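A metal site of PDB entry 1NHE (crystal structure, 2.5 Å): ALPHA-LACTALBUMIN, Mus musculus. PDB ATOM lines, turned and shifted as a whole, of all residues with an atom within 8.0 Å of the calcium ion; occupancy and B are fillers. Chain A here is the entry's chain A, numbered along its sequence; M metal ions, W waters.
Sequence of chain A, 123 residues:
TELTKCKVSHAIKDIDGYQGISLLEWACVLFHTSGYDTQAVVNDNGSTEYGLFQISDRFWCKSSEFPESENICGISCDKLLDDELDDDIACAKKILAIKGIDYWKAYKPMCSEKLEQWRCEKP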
ATOM      1  N   THR A  38       6.827  20.772  27.638  1.00  0.00           N
ATOM      2  CA  THR A  38       5.403  21.023  27.456  1.00  0.00           C
ATOM      3  C   THR A  38       4.881  22.322  28.087  1.00  0.00           C
ATOM      4  O   THR A  38       3.788  22.788  27.748  1.00  0.00           O
ATOM      5  CB  THR A  38       4.568  19.871  28.025  1.00  0.00           C
ATOM      6  OG1 THR A  38       4.712  19.849  29.460  1.00  0.00           O
ATOM      7  CG2 THR A  38       5.026  18.551  27.442  1.00  0.00           C
ATOM      8  N   GLY A  51       4.044  25.886  24.705  1.00  0.00           N
ATOM      9  CA  GLY A  51       4.269  24.469  24.748  1.00  0.00           C
ATOM     10  C   GLY A  51       5.363  23.837  23.946  1.00  0.00           C
ATOM     11  O   GLY A  51       6.264  24.507  23.451  1.00  0.00           O
ATOM     12  N   ILE A  75      -8.404  27.269  20.227  1.00  0.00           N
ATOM     13  CA  ILE A  75      -8.079  26.730  21.538  1.00  0.00           C
ATOM     14  C   ILE A  75      -7.451  27.802  22.393  1.00  0.00           C
ATOM     15  O   ILE A  75      -6.898  28.797  21.902  1.00  0.00           O
ATOM     16  CB  ILE A  75      -7.075  25.549  21.466  1.00  0.00           C
ATOM     17  CG1 ILE A  75      -5.691  26.066  21.084  1.00  0.00           C
ATOM     18  CG2 ILE A  75      -7.538  24.517  20.451  1.00  0.00           C
ATOM     19  CD1 ILE A  75      -4.681  24.955  20.935  1.00  0.00           C
ATOM     20  N   SER A  76      -7.544  27.592  23.693  1.00  0.00           N
ATOM     21  CA  SER A  76      -6.961  28.516  24.644  1.00  0.00           C
ATOM     22  C   SER A  76      -5.480  28.173  24.666  1.00  0.00           C
ATOM     23  O   SER A  76      -5.119  27.003  24.830  1.00  0.00           O
ATOM     24  CB  SER A  76      -7.600  28.284  26.016  1.00  0.00           C
ATOM     25  OG  SER A  76      -7.035  29.141  26.989  1.00  0.00           O
ATOM     26  N   CYS A  77      -4.615  29.157  24.473  1.00  0.00           N
ATOM     27  CA  CYS A  77      -3.180  28.855  24.492  1.00  0.00           C
ATOM     28  C   CYS A  77      -2.778  28.055  25.754  1.00  0.00           C
ATOM     29  O   CYS A  77      -1.943  27.142  25.670  1.00  0.00           O
ATOM     30  CB  CYS A  77      -2.324  30.135  24.379  1.00  0.00           C
ATOM     31  SG  CYS A  77      -2.434  31.128  22.822  1.00  0.00           S
ATOM     32  N   ASP A  78      -3.384  28.377  26.900  1.00  0.00           N
ATOM     33  CA  ASP A  78      -3.099  27.664  28.146  1.00  0.00           C
ATOM     34  C   ASP A  78      -3.253  26.148  28.043  1.00  0.00           C
ATOM     35  O   ASP A  78      -2.564  25.414  28.732  1.00  0.00           O
ATOM     36  CB  ASP A  78      -3.990  28.157  29.291  1.00  0.00           C
ATOM     37  CG  ASP A  78      -3.812  29.637  29.574  1.00  0.00           C
ATOM     38  OD1 ASP A  78      -2.652  30.105  29.610  1.00  0.00           O
ATOM     39  OD2 ASP A  78      -4.842  30.329  29.767  1.00  0.00           O
ATOM     40  N   LYS A  79      -4.148  25.665  27.197  1.00  0.00           N
ATOM     41  CA  LYS A  79      -4.337  24.220  27.025  1.00  0.00           C
ATOM     42  C   LYS A  79      -3.137  23.584  26.332  1.00  0.00           C
ATOM     43  O   LYS A  79      -3.058  22.359  26.174  1.00  0.00           O
ATOM     44  CB  LYS A  79      -5.606  23.938  26.211  1.00  0.00           C
ATOM     45  CG  LYS A  79      -6.844  23.551  27.038  1.00  0.00           C
ATOM     46  CD  LYS A  79      -7.390  24.691  27.898  1.00  0.00           C
ATOM     47  CE  LYS A  79      -8.081  24.125  29.150  1.00  0.00           C
ATOM     48  NZ  LYS A  79      -7.120  23.295  29.954  1.00  0.00           N
ATOM     49  N   LEU A  80      -2.193  24.427  25.915  1.00  0.00           N
ATOM     50  CA  LEU A  80      -0.989  23.964  25.258  1.00  0.00           C
ATOM     51  C   LEU A  80       0.173  23.861  26.256  1.00  0.00           C
ATOM     52  O   LEU A  80       1.292  23.486  25.887  1.00  0.00           O
ATOM     53  CB  LEU A  80      -0.637  24.912  24.119  1.00  0.00           C
ATOM     54  CG  LEU A  80      -1.614  24.918  22.935  1.00  0.00           C
ATOM     55  CD1 LEU A  80      -1.427  26.202  22.112  1.00  0.00           C
ATOM     56  CD2 LEU A  80      -1.395  23.664  22.085  1.00  0.00           C
ATOM     57  N   LEU A  81      -0.117  24.162  27.526  1.00  0.00           N
ATOM     58  CA  LEU A  81       0.876  24.104  28.574  1.00  0.00           C
ATOM     59  C   LEU A  81       0.691  22.922  29.525  1.00  0.00           C
ATOM     60  O   LEU A  81       1.427  22.789  30.498  1.00  0.00           O
ATOM     61  CB  LEU A  81       0.857  25.408  29.365  1.00  0.00           C
ATOM     62  CG  LEU A  81       1.141  26.672  28.557  1.00  0.00           C
ATOM     63  CD1 LEU A  81       1.043  27.916  29.427  1.00  0.00           C
ATOM     64  CD2 LEU A  81       2.537  26.585  27.980  1.00  0.00           C
ATOM     65  N   ASP A  82      -0.274  22.053  29.259  1.00  0.00           N
ATOM     66  CA  ASP A  82      -0.468  20.909  30.141  1.00  0.00           C
ATOM     67  C   ASP A  82       0.296  19.746  29.583  1.00  0.00           C
ATOM     68  O   ASP A  82       1.169  19.966  28.763  1.00  0.00           O
ATOM     69  CB  ASP A  82      -1.952  20.568  30.290  1.00  0.00           C
ATOM     70  CG  ASP A  82      -2.631  20.287  28.977  1.00  0.00           C
ATOM     71  OD1 ASP A  82      -2.131  19.442  28.219  1.00  0.00           O
ATOM     72  OD2 ASP A  82      -3.687  20.904  28.724  1.00  0.00           O
ATOM     73  N   ASP A  83      -0.005  18.520  29.992  1.00  0.00           N
ATOM     74  CA  ASP A  83       0.729  17.366  29.505  1.00  0.00           C
ATOM     75  C   ASP A  83      -0.024  16.481  28.561  1.00  0.00           C
ATOM     76  O   ASP A  83       0.392  15.354  28.269  1.00  0.00           O
ATOM     77  CB  ASP A  83       1.271  16.544  30.681  1.00  0.00           C
ATOM     78  CG  ASP A  83       2.507  17.177  31.315  1.00  0.00           C
ATOM     79  OD1 ASP A  83       2.596  18.429  31.368  1.00  0.00           O
ATOM     80  OD2 ASP A  83       3.396  16.422  31.761  1.00  0.00           O
ATOM     81  N   GLU A  84      -1.167  17.004  28.083  1.00  0.00           N
ATOM     82  CA  GLU A  84      -1.980  16.320  27.088  1.00  0.00           C
ATOM     83  C   GLU A  84      -1.645  17.011  25.783  1.00  0.00           C
ATOM     84  O   GLU A  84      -1.952  18.191  25.572  1.00  0.00           O
ATOM     85  CB  GLU A  84      -3.462  16.424  27.417  1.00  0.00           C
ATOM     86  CG  GLU A  84      -3.913  15.257  28.248  1.00  0.00           C
ATOM     87  CD  GLU A  84      -5.416  15.100  28.352  1.00  0.00           C
ATOM     88  OE1 GLU A  84      -6.110  15.107  27.292  1.00  0.00           O
ATOM     89  OE2 GLU A  84      -5.893  14.950  29.501  1.00  0.00           O
ATOM     90  N   LEU A  85      -1.011  16.250  24.908  1.00  0.00           N
ATOM     91  CA  LEU A  85      -0.524  16.768  23.637  1.00  0.00           C
ATOM     92  C   LEU A  85      -1.469  16.706  22.443  1.00  0.00           C
ATOM     93  O   LEU A  85      -1.237  17.375  21.431  1.00  0.00           O
ATOM     94  CB  LEU A  85       0.819  16.082  23.324  1.00  0.00           C
ATOM     95  CG  LEU A  85       2.068  16.725  23.971  1.00  0.00           C
ATOM     96  CD1 LEU A  85       1.712  17.313  25.288  1.00  0.00           C
ATOM     97  CD2 LEU A  85       3.176  15.719  24.110  1.00  0.00           C
ATOM     98  N   ASP A  86      -2.537  15.925  22.563  1.00  0.00           N
ATOM     99  CA  ASP A  86      -3.498  15.758  21.483  1.00  0.00           C
ATOM    100  C   ASP A  86      -3.923  17.051  20.804  1.00  0.00           C
ATOM    101  O   ASP A  86      -3.898  17.169  19.577  1.00  0.00           O
ATOM    102  CB  ASP A  86      -4.731  15.039  22.007  1.00  0.00           C
ATOM    103  CG  ASP A  86      -4.372  13.766  22.737  1.00  0.00           C
ATOM    104  OD1 ASP A  86      -4.135  13.834  23.977  1.00  0.00           O
ATOM    105  OD2 ASP A  86      -4.304  12.709  22.055  1.00  0.00           O
ATOM    106  N   ASP A  87      -4.300  18.030  21.608  1.00  0.00           N
ATOM    107  CA  ASP A  87      -4.726  19.291  21.049  1.00  0.00           C
ATOM    108  C   ASP A  87      -3.536  20.110  20.475  1.00  0.00           C
ATOM    109  O   ASP A  87      -3.719  20.898  19.536  1.00  0.00           O
ATOM    110  CB  ASP A  87      -5.523  20.071  22.102  1.00  0.00           C
ATOM    111  CG  ASP A  87      -4.776  20.239  23.390  1.00  0.00           C
ATOM    112  OD1 ASP A  87      -3.648  19.690  23.501  1.00  0.00           O
ATOM    113  OD2 ASP A  87      -5.309  20.922  24.291  1.00  0.00           O
ATOM    114  N   ASP A  88      -2.336  19.911  21.028  1.00  0.00           N
ATOM    115  CA  ASP A  88      -1.125  20.581  20.550  1.00  0.00           C
ATOM    116  C   ASP A  88      -0.799  19.968  19.202  1.00  0.00           C
ATOM    117  O   ASP A  88      -0.369  20.662  18.282  1.00  0.00           O
ATOM    118  CB  ASP A  88       0.059  20.324  21.487  1.00  0.00           C
ATOM    119  CG  ASP A  88      -0.278  20.558  22.936  1.00  0.00           C
ATOM    120  OD1 ASP A  88       0.345  21.448  23.552  1.00  0.00           O
ATOM    121  OD2 ASP A  88      -1.172  19.857  23.464  1.00  0.00           O
ATOM    122  N   ILE A  89      -1.003  18.669  19.091  1.00  0.00           N
ATOM    123  CA  ILE A  89      -0.748  17.982  17.854  1.00  0.00           C
ATOM    124  C   ILE A  89      -1.730  18.383  16.783  1.00  0.00           C
ATOM    125  O   ILE A  89      -1.369  18.572  15.637  1.00  0.00           O
ATOM    126  CB  ILE A  89      -0.833  16.452  18.033  1.00  0.00           C
ATOM    127  CG1 ILE A  89       0.296  15.988  18.979  1.00  0.00           C
ATOM    128  CG2 ILE A  89      -0.756  15.757  16.673  1.00  0.00           C
ATOM    129  CD1 ILE A  89       0.400  14.491  19.122  1.00  0.00           C
HETATM  130 CA    CA M   1      -2.479  20.376  25.559  1.00  0.00          CA
HETATM  131  O   HOH W   1       0.043  20.834  26.485  1.00  0.00           O
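Residues that only touch the calcium ion: Leu 80 (3.9 Å). The nearest printed residue that does not touch the calcium ion is Leu 85 (4.4 Å).
The calcium ion is bound by O of Lys 79 (2.2 Å). The backbone carbonyl oxygen (O) of Glu 84 is bound to the calcium ion, 2.2 Å away. The calcium ion is bound by OD1 of Asp 87. The side-chain carboxylate (OD2) of Asp 88 is bound to the calcium ion, 2.5 Å away. The calcium ion is bound by water W1. OD1 of Asp 82 binds the calcium ion (2.8 Å). The calcium ion has six donor atoms within binding distance. Slightly farther from the calcium ion lies the side-chain carboxylate (OD2) of Asp 87 (3.1 Å).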
